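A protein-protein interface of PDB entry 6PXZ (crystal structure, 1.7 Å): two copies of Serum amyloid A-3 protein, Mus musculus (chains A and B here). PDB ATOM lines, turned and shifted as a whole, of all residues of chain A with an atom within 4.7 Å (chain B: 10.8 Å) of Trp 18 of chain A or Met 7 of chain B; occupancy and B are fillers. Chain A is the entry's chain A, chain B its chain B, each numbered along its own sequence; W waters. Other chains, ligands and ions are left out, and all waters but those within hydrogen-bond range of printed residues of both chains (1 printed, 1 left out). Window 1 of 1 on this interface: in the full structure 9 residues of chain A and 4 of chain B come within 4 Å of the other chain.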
ATOM      1  N   SER A  14      -8.671 -24.974   0.144  1.00  0.00           N
ATOM      2  CA  SER A  14      -8.090 -24.572  -1.133  1.00  0.00           C
ATOM      3  C   SER A  14      -8.218 -23.065  -1.290  1.00  0.00           C
ATOM      4  O   SER A  14      -7.281 -22.388  -1.714  1.00  0.00           O
ATOM      5  CB  SER A  14      -8.789 -25.300  -2.284  1.00  0.00           C
ATOM      6  OG  SER A  14      -8.522 -26.686  -2.200  1.00  0.00           O
ATOM      7  N   ARG A  15      -9.387 -22.539  -0.940  1.00  0.00           N
ATOM      8  CA  ARG A  15      -9.614 -21.100  -0.990  1.00  0.00           C
ATOM      9  C   ARG A  15      -8.681 -20.338  -0.047  1.00  0.00           C
ATOM     10  O   ARG A  15      -8.226 -19.251  -0.382  1.00  0.00           O
ATOM     11  CB  ARG A  15     -11.082 -20.773  -0.678  1.00  0.00           C
ATOM     12  CG  ARG A  15     -12.068 -21.275  -1.734  1.00  0.00           C
ATOM     13  CD  ARG A  15     -13.492 -20.718  -1.519  1.00  0.00           C
ATOM     14  NE  ARG A  15     -14.215 -21.332  -0.400  1.00  0.00           N
ATOM     15  CZ  ARG A  15     -14.595 -20.692   0.712  1.00  0.00           C
ATOM     16  NH1 ARG A  15     -14.319 -19.403   0.885  1.00  0.00           N
ATOM     17  NH2 ARG A  15     -15.253 -21.346   1.661  1.00  0.00           N
ATOM     18  N   ASP A  16      -8.401 -20.916   1.122  1.00  0.00           N
ATOM     19  CA  ASP A  16      -7.453 -20.350   2.080  1.00  0.00           C
ATOM     20  C   ASP A  16      -6.045 -20.274   1.494  1.00  0.00           C
ATOM     21  O   ASP A  16      -5.298 -19.320   1.744  1.00  0.00           O
ATOM     22  CB  ASP A  16      -7.395 -21.202   3.359  1.00  0.00           C
ATOM     23  CG  ASP A  16      -8.623 -21.041   4.236  1.00  0.00           C
ATOM     24  OD1 ASP A  16      -9.240 -19.957   4.218  1.00  0.00           O
ATOM     25  OD2 ASP A  16      -8.949 -22.000   4.962  1.00  0.00           O
ATOM     26  N   MET A  17      -5.676 -21.298   0.734  1.00  0.00           N
ATOM     27  CA  MET A  17      -4.368 -21.305   0.093  1.00  0.00           C
ATOM     28  C   MET A  17      -4.272 -20.229  -0.979  1.00  0.00           C
ATOM     29  O   MET A  17      -3.282 -19.511  -1.037  1.00  0.00           O
ATOM     30  CB  MET A  17      -4.030 -22.689  -0.478  1.00  0.00           C
ATOM     31  CG  MET A  17      -3.834 -23.769   0.593  1.00  0.00           C
ATOM     32  SD  MET A  17      -2.389 -23.531   1.660  1.00  0.00           S
ATOM     33  CE  MET A  17      -1.054 -23.884   0.503  1.00  0.00           C
ATOM     34  N   TRP A  18      -5.292 -20.099  -1.821  1.00  0.00           N
ATOM     35  CA  TRP A  18      -5.234 -19.079  -2.871  1.00  0.00           C
ATOM     36  C   TRP A  18      -5.254 -17.699  -2.246  1.00  0.00           C
ATOM     37  O   TRP A  18      -4.620 -16.786  -2.749  1.00  0.00           O
ATOM     38  CB  TRP A  18      -6.391 -19.194  -3.879  1.00  0.00           C
ATOM     39  CG  TRP A  18      -6.744 -20.600  -4.319  1.00  0.00           C
ATOM     40  CD1 TRP A  18      -7.999 -21.121  -4.414  1.00  0.00           C
ATOM     41  CD2 TRP A  18      -5.846 -21.645  -4.732  1.00  0.00           C
ATOM     42  NE1 TRP A  18      -7.944 -22.422  -4.851  1.00  0.00           N
ATOM     43  CE2 TRP A  18      -6.635 -22.769  -5.053  1.00  0.00           C
ATOM     44  CE3 TRP A  18      -4.456 -21.741  -4.860  1.00  0.00           C
ATOM     45  CZ2 TRP A  18      -6.084 -23.974  -5.484  1.00  0.00           C
ATOM     46  CZ3 TRP A  18      -3.908 -22.947  -5.294  1.00  0.00           C
ATOM     47  CH2 TRP A  18      -4.720 -24.039  -5.598  1.00  0.00           C
ATOM     48  N   ARG A  19      -5.978 -17.546  -1.144  1.00  0.00           N
ATOM     49  CA  ARG A  19      -6.040 -16.240  -0.483  1.00  0.00           C
ATOM     50  C   ARG A  19      -4.664 -15.873   0.063  1.00  0.00           C
ATOM     51  O   ARG A  19      -4.230 -14.715  -0.006  1.00  0.00           O
ATOM     52  CB  ARG A  19      -7.113 -16.219   0.618  1.00  0.00           C
ATOM     53  CG  ARG A  19      -7.301 -14.839   1.260  1.00  0.00           C
ATOM     54  CD  ARG A  19      -8.541 -14.833   2.158  1.00  0.00           C
ATOM     55  NE  ARG A  19      -8.613 -16.056   2.957  1.00  0.00           N
ATOM     56  CZ  ARG A  19      -8.015 -16.211   4.136  1.00  0.00           C
ATOM     57  NH1 ARG A  19      -7.311 -15.217   4.655  1.00  0.00           N
ATOM     58  NH2 ARG A  19      -8.116 -17.362   4.790  1.00  0.00           N
ATOM     59  N   ALA A  20      -3.946 -16.870   0.563  1.00  0.00           N
ATOM     60  CA  ALA A  20      -2.607 -16.616   1.068  1.00  0.00           C
ATOM     61  C   ALA A  20      -1.661 -16.216  -0.062  1.00  0.00           C
ATOM     62  O   ALA A  20      -0.818 -15.335   0.104  1.00  0.00           O
ATOM     63  CB  ALA A  20      -2.071 -17.833   1.804  1.00  0.00           C
ATOM     64  N   TYR A  21      -1.783 -16.876  -1.213  1.00  0.00           N
ATOM     65  CA  TYR A  21      -0.902 -16.561  -2.338  1.00  0.00           C
ATOM     66  C   TYR A  21      -1.283 -15.178  -2.896  1.00  0.00           C
ATOM     67  O   TYR A  21      -0.419 -14.390  -3.283  1.00  0.00           O
ATOM     68  CB  TYR A  21      -0.995 -17.656  -3.407  1.00  0.00           C
ATOM     69  CG  TYR A  21      -0.446 -19.026  -2.990  1.00  0.00           C
ATOM     70  CD1 TYR A  21       0.640 -19.148  -2.125  1.00  0.00           C
ATOM     71  CD2 TYR A  21      -1.022 -20.201  -3.477  1.00  0.00           C
ATOM     72  CE1 TYR A  21       1.144 -20.405  -1.765  1.00  0.00           C
ATOM     73  CE2 TYR A  21      -0.527 -21.459  -3.117  1.00  0.00           C
ATOM     74  CZ  TYR A  21       0.543 -21.551  -2.264  1.00  0.00           C
ATOM     75  OH  TYR A  21       1.030 -22.796  -1.920  1.00  0.00           O
ATOM     76  N   SER A  22      -2.583 -14.898  -2.913  1.00  0.00           N
ATOM     77  CA  SER A  22      -3.102 -13.616  -3.359  1.00  0.00           C
ATOM     78  C   SER A  22      -2.618 -12.487  -2.447  1.00  0.00           C
ATOM     79  O   SER A  22      -2.147 -11.451  -2.928  1.00  0.00           O
ATOM     80  CB  SER A  22      -4.629 -13.654  -3.396  1.00  0.00           C
ATOM     81  OG  SER A  22      -5.150 -12.412  -3.818  1.00  0.00           O
ATOM     82  N   ILE A  58      -1.768 -29.047  -2.367  1.00  0.00           N
ATOM     83  CA  ILE A  58      -1.376 -27.821  -3.028  1.00  0.00           C
ATOM     84  C   ILE A  58       0.084 -27.510  -2.742  1.00  0.00           C
ATOM     85  O   ILE A  58       0.812 -27.148  -3.662  1.00  0.00           O
ATOM     86  CB  ILE A  58      -2.277 -26.645  -2.609  1.00  0.00           C
ATOM     87  CG1 ILE A  58      -3.647 -26.788  -3.271  1.00  0.00           C
ATOM     88  CG2 ILE A  58      -1.663 -25.319  -3.008  1.00  0.00           C
ATOM     89  CD1 ILE A  58      -4.715 -25.968  -2.589  1.00  0.00           C
ATOM     90  N   ALA A  61       2.199 -30.064  -4.633  1.00  0.00           N
ATOM     91  CA  ALA A  61       2.182 -29.762  -6.061  1.00  0.00           C
ATOM     92  C   ALA A  61       3.129 -28.611  -6.383  1.00  0.00           C
ATOM     93  O   ALA A  61       3.825 -28.626  -7.408  1.00  0.00           O
ATOM     94  CB  ALA A  61       0.789 -29.441  -6.523  1.00  0.00           C
ATOM     95  N   ARG B   2       0.412 -19.041 -14.937  1.00  0.00           N
ATOM     96  CA  ARG B   2       0.814 -19.375 -13.575  1.00  0.00           C
ATOM     97  C   ARG B   2       0.442 -20.812 -13.194  1.00  0.00           C
ATOM     98  O   ARG B   2      -0.549 -21.386 -13.683  1.00  0.00           O
ATOM     99  CB  ARG B   2       0.187 -18.398 -12.565  1.00  0.00           C
ATOM    100  CG  ARG B   2       0.989 -17.111 -12.341  1.00  0.00           C
ATOM    101  CD  ARG B   2       1.830 -17.170 -11.077  1.00  0.00           C
ATOM    102  NE  ARG B   2       3.006 -18.029 -11.221  1.00  0.00           N
ATOM    103  CZ  ARG B   2       3.867 -18.303 -10.243  1.00  0.00           C
ATOM    104  NH1 ARG B   2       3.674 -17.808  -9.023  1.00  0.00           N
ATOM    105  NH2 ARG B   2       4.906 -19.093 -10.480  1.00  0.00           N
ATOM    106  N   TRP B   3       1.259 -21.385 -12.322  1.00  0.00           N
ATOM    107  CA  TRP B   3       0.905 -22.610 -11.631  1.00  0.00           C
ATOM    108  C   TRP B   3      -0.346 -22.360 -10.792  1.00  0.00           C
ATOM    109  O   TRP B   3      -1.217 -23.223 -10.710  1.00  0.00           O
ATOM    110  CB  TRP B   3       2.067 -23.073 -10.752  1.00  0.00           C
ATOM    111  CG  TRP B   3       1.688 -24.116  -9.730  1.00  0.00           C
ATOM    112  CD1 TRP B   3       1.566 -25.462  -9.928  1.00  0.00           C
ATOM    113  CD2 TRP B   3       1.422 -23.890  -8.342  1.00  0.00           C
ATOM    114  NE1 TRP B   3       1.221 -26.083  -8.746  1.00  0.00           N
ATOM    115  CE2 TRP B   3       1.130 -25.137  -7.759  1.00  0.00           C
ATOM    116  CE3 TRP B   3       1.395 -22.747  -7.536  1.00  0.00           C
ATOM    117  CZ2 TRP B   3       0.811 -25.273  -6.404  1.00  0.00           C
ATOM    118  CZ3 TRP B   3       1.081 -22.881  -6.195  1.00  0.00           C
ATOM    119  CH2 TRP B   3       0.786 -24.132  -5.644  1.00  0.00           C
ATOM    120  N   VAL B   4      -0.442 -21.187 -10.170  1.00  0.00           N
ATOM    121  CA  VAL B   4      -1.628 -20.867  -9.375  1.00  0.00           C
ATOM    122  C   VAL B   4      -2.920 -20.956 -10.193  1.00  0.00           C
ATOM    123  O   VAL B   4      -3.903 -21.553  -9.743  1.00  0.00           O
ATOM    124  CB  VAL B   4      -1.532 -19.471  -8.698  1.00  0.00           C
ATOM    125  CG1 VAL B   4      -2.875 -19.067  -8.139  1.00  0.00           C
ATOM    126  CG2 VAL B   4      -0.483 -19.482  -7.597  1.00  0.00           C
ATOM    127  N   GLN B   5      -2.918 -20.389 -11.399  1.00  0.00           N
ATOM    128  CA  GLN B   5      -4.130 -20.401 -12.217  1.00  0.00           C
ATOM    129  C   GLN B   5      -4.527 -21.823 -12.611  1.00  0.00           C
ATOM    130  O   GLN B   5      -5.702 -22.192 -12.543  1.00  0.00           O
ATOM    131  CB  GLN B   5      -3.974 -19.538 -13.471  1.00  0.00           C
ATOM    132  CG  GLN B   5      -5.300 -19.302 -14.195  1.00  0.00           C
ATOM    133  CD  GLN B   5      -6.459 -18.989 -13.242  1.00  0.00           C
ATOM    134  OE1 GLN B   5      -7.455 -19.731 -13.182  1.00  0.00           O
ATOM    135  NE2 GLN B   5      -6.341 -17.887 -12.499  1.00  0.00           N
ATOM    136  N   PHE B   6      -3.533 -22.605 -13.017  1.00  0.00           N
ATOM    137  CA  PHE B   6      -3.722 -24.018 -13.309  1.00  0.00           C
ATOM    138  C   PHE B   6      -4.300 -24.727 -12.094  1.00  0.00           C
ATOM    139  O   PHE B   6      -5.236 -25.517 -12.229  1.00  0.00           O
ATOM    140  CB  PHE B   6      -2.374 -24.645 -13.712  1.00  0.00           C
ATOM    141  CG  PHE B   6      -2.455 -26.107 -14.076  1.00  0.00           C
ATOM    142  CD1 PHE B   6      -2.327 -27.089 -13.102  1.00  0.00           C
ATOM    143  CD2 PHE B   6      -2.628 -26.500 -15.397  1.00  0.00           C
ATOM    144  CE1 PHE B   6      -2.393 -28.449 -13.438  1.00  0.00           C
ATOM    145  CE2 PHE B   6      -2.692 -27.853 -15.735  1.00  0.00           C
ATOM    146  CZ  PHE B   6      -2.575 -28.822 -14.748  1.00  0.00           C
ATOM    147  N   MET B   7      -3.764 -24.458 -10.901  1.00  0.00           N
ATOM    148  CA  MET B   7      -4.242 -25.191  -9.723  1.00  0.00           C
ATOM    149  C   MET B   7      -5.664 -24.809  -9.363  1.00  0.00           C
ATOM    150  O   MET B   7      -6.430 -25.633  -8.867  1.00  0.00           O
ATOM    151  CB  MET B   7      -3.337 -24.986  -8.510  1.00  0.00           C
ATOM    152  CG  MET B   7      -2.014 -25.685  -8.607  1.00  0.00           C
ATOM    153  SD  MET B   7      -2.065 -27.471  -8.855  1.00  0.00           S
ATOM    154  CE  MET B   7      -2.641 -28.035  -7.258  1.00  0.00           C
ATOM    155  N   LYS B   8      -6.006 -23.543  -9.595  1.00  0.00           N
ATOM    156  CA  LYS B   8      -7.370 -23.091  -9.383  1.00  0.00           C
ATOM    157  C   LYS B   8      -8.306 -23.817 -10.324  1.00  0.00           C
ATOM    158  O   LYS B   8      -9.366 -24.270  -9.899  1.00  0.00           O
ATOM    159  CB  LYS B   8      -7.467 -21.581  -9.577  1.00  0.00           C
ATOM    160  CG  LYS B   8      -6.892 -20.822  -8.404  1.00  0.00           C
ATOM    161  CD  LYS B   8      -6.903 -19.324  -8.666  1.00  0.00           C
ATOM    162  CE  LYS B   8      -6.370 -18.556  -7.458  1.00  0.00           C
ATOM    163  NZ  LYS B   8      -6.483 -17.082  -7.660  1.00  0.00           N
ATOM    164  N   GLU B   9      -7.910 -23.939 -11.588  1.00  0.00           N
ATOM    165  CA  GLU B   9      -8.704 -24.717 -12.549  1.00  0.00           C
ATOM    166  C   GLU B   9      -8.849 -26.159 -12.084  1.00  0.00           C
ATOM    167  O   GLU B   9      -9.924 -26.743 -12.197  1.00  0.00           O
ATOM    168  CB  GLU B   9      -8.084 -24.667 -13.954  1.00  0.00           C
ATOM    169  CG  GLU B   9      -8.142 -23.278 -14.581  1.00  0.00           C
ATOM    170  CD  GLU B   9      -7.202 -23.103 -15.760  1.00  0.00           C
ATOM    171  OE1 GLU B   9      -6.452 -24.054 -16.096  1.00  0.00           O
ATOM    172  OE2 GLU B   9      -7.207 -22.003 -16.360  1.00  0.00           O
ATOM    173  N   ALA B  10      -7.766 -26.733 -11.559  1.00  0.00           N
ATOM    174  CA  ALA B  10      -7.806 -28.110 -11.065  1.00  0.00           C
ATOM    175  C   ALA B  10      -8.797 -28.277  -9.919  1.00  0.00           C
ATOM    176  O   ALA B  10      -9.525 -29.260  -9.878  1.00  0.00           O
ATOM    177  CB  ALA B  10      -6.425 -28.565 -10.635  1.00  0.00           C
ATOM    178  N   GLY B  11      -8.809 -27.319  -8.991  1.00  0.00           N
ATOM    179  CA  GLY B  11      -9.738 -27.318  -7.879  1.00  0.00           C
ATOM    180  C   GLY B  11     -11.169 -27.254  -8.366  1.00  0.00           C
ATOM    181  O   GLY B  11     -12.039 -27.963  -7.862  1.00  0.00           O
ATOM    182  N   GLN B  12     -11.426 -26.410  -9.362  1.00  0.00           N
ATOM    183  CA  GLN B  12     -12.790 -26.289  -9.870  1.00  0.00           C
ATOM    184  C   GLN B  12     -13.209 -27.558 -10.603  1.00  0.00           C
ATOM    185  O   GLN B  12     -14.336 -28.020 -10.468  1.00  0.00           O
ATOM    186  CB  GLN B  12     -12.908 -25.098 -10.811  1.00  0.00           C
ATOM    187  CG  GLN B  12     -12.803 -23.739 -10.109  1.00  0.00           C
ATOM    188  CD  GLN B  12     -12.613 -22.619 -11.108  1.00  0.00           C
ATOM    189  OE1 GLN B  12     -11.973 -22.802 -12.153  1.00  0.00           O
ATOM    190  NE2 GLN B  12     -13.175 -21.447 -10.800  1.00  0.00           N
ATOM    191  N   GLY B  13     -12.293 -28.105 -11.384  1.00  0.00           N
ATOM    192  CA  GLY B  13     -12.574 -29.341 -12.094  1.00  0.00           C
ATOM    193  C   GLY B  13     -12.808 -30.483 -11.135  1.00  0.00           C
ATOM    194  O   GLY B  13     -13.623 -31.356 -11.395  1.00  0.00           O
ATOM    195  N   SER B  14     -12.089 -30.493 -10.020  1.00  0.00           N
ATOM    196  CA  SER B  14     -12.316 -31.512  -9.006  1.00  0.00           C
ATOM    197  C   SER B  14     -13.720 -31.386  -8.451  1.00  0.00           C
ATOM    198  O   SER B  14     -14.413 -32.385  -8.257  1.00  0.00           O
ATOM    199  CB  SER B  14     -11.286 -31.384  -7.881  1.00  0.00           C
ATOM    200  OG  SER B  14      -9.987 -31.648  -8.385  1.00  0.00           O
ATOM    201  N   ARG B  15     -14.142 -30.153  -8.206  1.00  0.00           N
ATOM    202  CA  ARG B  15     -15.504 -29.913  -7.740  1.00  0.00           C
ATOM    203  C   ARG B  15     -16.511 -30.421  -8.770  1.00  0.00           C
ATOM    204  O   ARG B  15     -17.518 -31.042  -8.417  1.00  0.00           O
ATOM    205  CB  ARG B  15     -15.724 -28.422  -7.456  1.00  0.00           C
ATOM    206  CG  ARG B  15     -17.181 -28.069  -7.205  1.00  0.00           C
ATOM    207  CD  ARG B  15     -17.476 -27.789  -5.741  1.00  0.00           C
ATOM    208  NE  ARG B  15     -16.926 -26.504  -5.305  1.00  0.00           N
ATOM    209  CZ  ARG B  15     -17.574 -25.339  -5.369  1.00  0.00           C
ATOM    210  NH1 ARG B  15     -18.808 -25.280  -5.855  1.00  0.00           N
ATOM    211  NH2 ARG B  15     -16.985 -24.227  -4.943  1.00  0.00           N
ATOM    212  N   ALA B  44     -15.398 -30.323 -16.119  1.00  0.00           N
ATOM    213  CA  ALA B  44     -14.047 -30.045 -15.612  1.00  0.00           C
ATOM    214  C   ALA B  44     -13.108 -29.514 -16.681  1.00  0.00           C
ATOM    215  O   ALA B  44     -12.365 -28.560 -16.438  1.00  0.00           O
ATOM    216  CB  ALA B  44     -13.446 -31.274 -14.959  1.00  0.00           C
ATOM    217  N   ARG B  47     -13.202 -25.880 -17.531  1.00  0.00           N
ATOM    218  CA  ARG B  47     -12.638 -24.922 -16.579  1.00  0.00           C
ATOM    219  C   ARG B  47     -11.299 -24.408 -17.083  1.00  0.00           C
ATOM    220  O   ARG B  47     -10.805 -23.378 -16.625  1.00  0.00           O
ATOM    221  CB  ARG B  47     -12.413 -25.581 -15.217  1.00  0.00           C
ATOM    222  CG  ARG B  47     -13.670 -26.082 -14.551  1.00  0.00           C
ATOM    223  CD  ARG B  47     -14.507 -24.940 -14.030  1.00  0.00           C
ATOM    224  NE  ARG B  47     -15.628 -25.449 -13.247  1.00  0.00           N
ATOM    225  CZ  ARG B  47     -16.478 -24.677 -12.582  1.00  0.00           C
ATOM    226  NH1 ARG B  47     -16.325 -23.362 -12.616  1.00  0.00           N
ATOM    227  NH2 ARG B  47     -17.473 -25.220 -11.896  1.00  0.00           N
ATOM    228  N   GLY B  48     -10.701 -25.131 -18.023  1.00  0.00           N
ATOM    229  CA  GLY B  48      -9.354 -24.814 -18.458  1.00  0.00           C
ATOM    230  C   GLY B  48      -8.420 -25.998 -18.279  1.00  0.00           C
ATOM    231  O   GLY B  48      -8.833 -27.040 -17.764  1.00  0.00           O
ATOM    232  N   PRO B  49      -7.149 -25.852 -18.692  1.00  0.00           N
ATOM    233  CA  PRO B  49      -6.184 -26.957 -18.660  1.00  0.00           C
ATOM    234  C   PRO B  49      -6.077 -27.644 -17.310  1.00  0.00           C
ATOM    235  O   PRO B  49      -5.945 -28.866 -17.280  1.00  0.00           O
ATOM    236  CB  PRO B  49      -4.865 -26.261 -18.984  1.00  0.00           C
ATOM    237  CG  PRO B  49      -5.284 -25.172 -19.934  1.00  0.00           C
ATOM    238  CD  PRO B  49      -6.630 -24.690 -19.434  1.00  0.00           C
ATOM    239  N   GLY B  50      -6.119 -26.882 -16.221  1.00  0.00           N
ATOM    240  CA  GLY B  50      -6.013 -27.477 -14.905  1.00  0.00           C
ATOM    241  C   GLY B  50      -7.200 -28.371 -14.623  1.00  0.00           C
ATOM    242  O   GLY B  50      -7.080 -29.381 -13.925  1.00  0.00           O
ATOM    243  N   GLY B  51      -8.352 -27.982 -15.155  1.00  0.00           N
ATOM    244  CA  GLY B  51      -9.575 -28.738 -14.929  1.00  0.00           C
ATOM    245  C   GLY B  51      -9.549 -30.037 -15.708  1.00  0.00           C
ATOM    246  O   GLY B  51      -9.987 -31.089 -15.228  1.00  0.00           O
ATOM    247  N   ALA B  52      -9.038 -29.971 -16.933  1.00  0.00           N
ATOM    248  CA  ALA B  52      -8.909 -31.178 -17.743  1.00  0.00           C
ATOM    249  C   ALA B  52      -7.936 -32.152 -17.084  1.00  0.00           C
ATOM    250  O   ALA B  52      -8.144 -33.369 -17.101  1.00  0.00           O
ATOM    251  CB  ALA B  52      -8.475 -30.839 -19.160  1.00  0.00           C
ATOM    252  N   TRP B  53      -6.870 -31.610 -16.496  1.00  0.00           N
ATOM    253  CA  TRP B  53      -5.890 -32.425 -15.800  1.00  0.00           C
ATOM    254  C   TRP B  53      -6.501 -33.132 -14.589  1.00  0.00           C
ATOM    255  O   TRP B  53      -6.333 -34.350 -14.407  1.00  0.00           O
ATOM    256  CB  TRP B  53      -4.714 -31.552 -15.370  1.00  0.00           C
ATOM    257  CG  TRP B  53      -3.764 -32.268 -14.494  1.00  0.00           C
ATOM    258  CD1 TRP B  53      -2.871 -33.234 -14.871  1.00  0.00           C
ATOM    259  CD2 TRP B  53      -3.616 -32.106 -13.089  1.00  0.00           C
ATOM    260  NE1 TRP B  53      -2.174 -33.674 -13.780  1.00  0.00           N
ATOM    261  CE2 TRP B  53      -2.613 -33.004 -12.668  1.00  0.00           C
ATOM    262  CE3 TRP B  53      -4.222 -31.281 -12.142  1.00  0.00           C
ATOM    263  CZ2 TRP B  53      -2.204 -33.098 -11.339  1.00  0.00           C
ATOM    264  CZ3 TRP B  53      -3.824 -31.379 -10.818  1.00  0.00           C
ATOM    265  CH2 TRP B  53      -2.819 -32.280 -10.429  1.00  0.00           C
ATOM    266  N   ALA B  54      -7.214 -32.371 -13.764  1.00  0.00           N
ATOM    267  CA  ALA B  54      -7.864 -32.941 -12.591  1.00  0.00           C
ATOM    268  C   ALA B  54      -8.828 -34.035 -13.027  1.00  0.00           C
ATOM    269  O   ALA B  54      -8.886 -35.090 -12.402  1.00  0.00           O
ATOM    270  CB  ALA B  54      -8.596 -31.855 -11.790  1.00  0.00           C
ATOM    271  N   ALA B  55      -9.586 -33.785 -14.092  1.00  0.00           N
ATOM    272  CA  ALA B  55     -10.555 -34.773 -14.568  1.00  0.00           C
ATOM    273  C   ALA B  55      -9.838 -36.062 -14.947  1.00  0.00           C
ATOM    274  O   ALA B  55     -10.299 -37.160 -14.625  1.00  0.00           O
ATOM    275  CB  ALA B  55     -11.361 -34.242 -15.745  1.00  0.00           C
ATOM    276  N   VAL B  57      -6.766 -37.147 -13.911  1.00  0.00           N
ATOM    277  CA  VAL B  57      -6.145 -37.739 -12.729  1.00  0.00           C
ATOM    278  C   VAL B  57      -7.195 -38.467 -11.875  1.00  0.00           C
ATOM    279  O   VAL B  57      -6.988 -39.595 -11.423  1.00  0.00           O
ATOM    280  CB  VAL B  57      -5.401 -36.650 -11.931  1.00  0.00           C
ATOM    281  CG1 VAL B  57      -5.090 -37.113 -10.533  1.00  0.00           C
ATOM    282  CG2 VAL B  57      -4.124 -36.245 -12.684  1.00  0.00           C
ATOM    283  N   ILE B  58      -8.343 -37.830 -11.690  1.00  0.00           N
ATOM    284  CA  ILE B  58      -9.435 -38.442 -10.944  1.00  0.00           C
ATOM    285  C   ILE B  58     -10.040 -39.638 -11.663  1.00  0.00           C
ATOM    286  O   ILE B  58     -10.279 -40.677 -11.048  1.00  0.00           O
ATOM    287  CB  ILE B  58     -10.517 -37.393 -10.617  1.00  0.00           C
ATOM    288  CG1 ILE B  58      -9.971 -36.404  -9.589  1.00  0.00           C
ATOM    289  CG2 ILE B  58     -11.791 -38.065 -10.115  1.00  0.00           C
ATOM    290  CD1 ILE B  58     -10.710 -35.044  -9.565  1.00  0.00           C
HETATM  291  O   HOH W   1      -4.320 -16.753  -5.477  1.00  0.00           O
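The indole nitrogen of Trp 18 of chain A lies close to the backbone carbonyl oxygen of Ser 14 of chain A (3.2 Å).
The indole nitrogen (NE1) of Trp 3 of chain B lies close to the side-chain sulfur (SD) of Met 7 of chain B (3.6 Å).
Among the printed residues, pairs that only touch across the chains: Ile 58 of chain A with Trp 3 of chain B (3.3 Å), Trp 18 of chain A with Met 7 of chain B (3.4 Å), Trp 18 of chain A with Lys 8 of chain B (3.6 Å), Tyr 21 of chain A with Trp 3 of chain B (3.8 Å), Ala 61 of chain A with Met 7 of chain B (3.8 Å) and Ala 61 of chain A with Trp 3 of chain B (3.9 Å).
Trp 18 of chain A touches just these residues of chain B: Met 7 (3.4 Å) and Lys 8 (3.6 Å).
Met 7 of chain B touches just these residues of chain A: Trp 18 (3.4 Å) and Ala 61 (3.8 Å).
No residue of chain B comes within 4 Å of Ala 20 of chain A.
Tyr 21 of chain A touches just one residue of chain B: Trp 3 (3.8 Å).
Of chain B, only Trp 3 comes within 4 Å of Ile 58 of chain A.
Ala 61 of chain A touches two residues of chain B.
Printed residues of chain A within 4 Å of Lys 8 of chain B: Trp 18.
Printed residues of chain A within 4 Å of Trp 3 of chain B: Tyr 21, Ile 58 and Ala 61.
Gly 50 of chain B touches none of the printed residues of chain A.
Asp 16 of chain A touches none of the printed residues of chain B.
The nearest residue of chain B that does not touch Trp 18 of chain A is Val 4 of chain B (4.5 Å).
The nearest residue of chain A that does not touch Met 7 of chain B is Ile 58 of chain A (4.3 Å).
The nearest printed residue of chain A that does not touch Trp 3 of chain B is Trp 18 of chain A (4.9 Å).
Of the 11 printed residues of chain A, 4 touch a printed residue of chain B.
Of the 26 printed residues of chain B, 3 touch a printed residue of chain A.
Hydrophobic or aromatic side chains of chain B within 4 Å of the printed part of chain A: Trp 3 and Met 7.
Among the printed residues, 6 pairs touch across the chains.
3 positions are printed for both chains.
Of the 6 pairs that touch across the chains among the printed residues, none has its exchanged pair printed and touching as well.
Water W1 bridges O of Trp 18 of chain A and NZ of Lys 8 of chain B.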
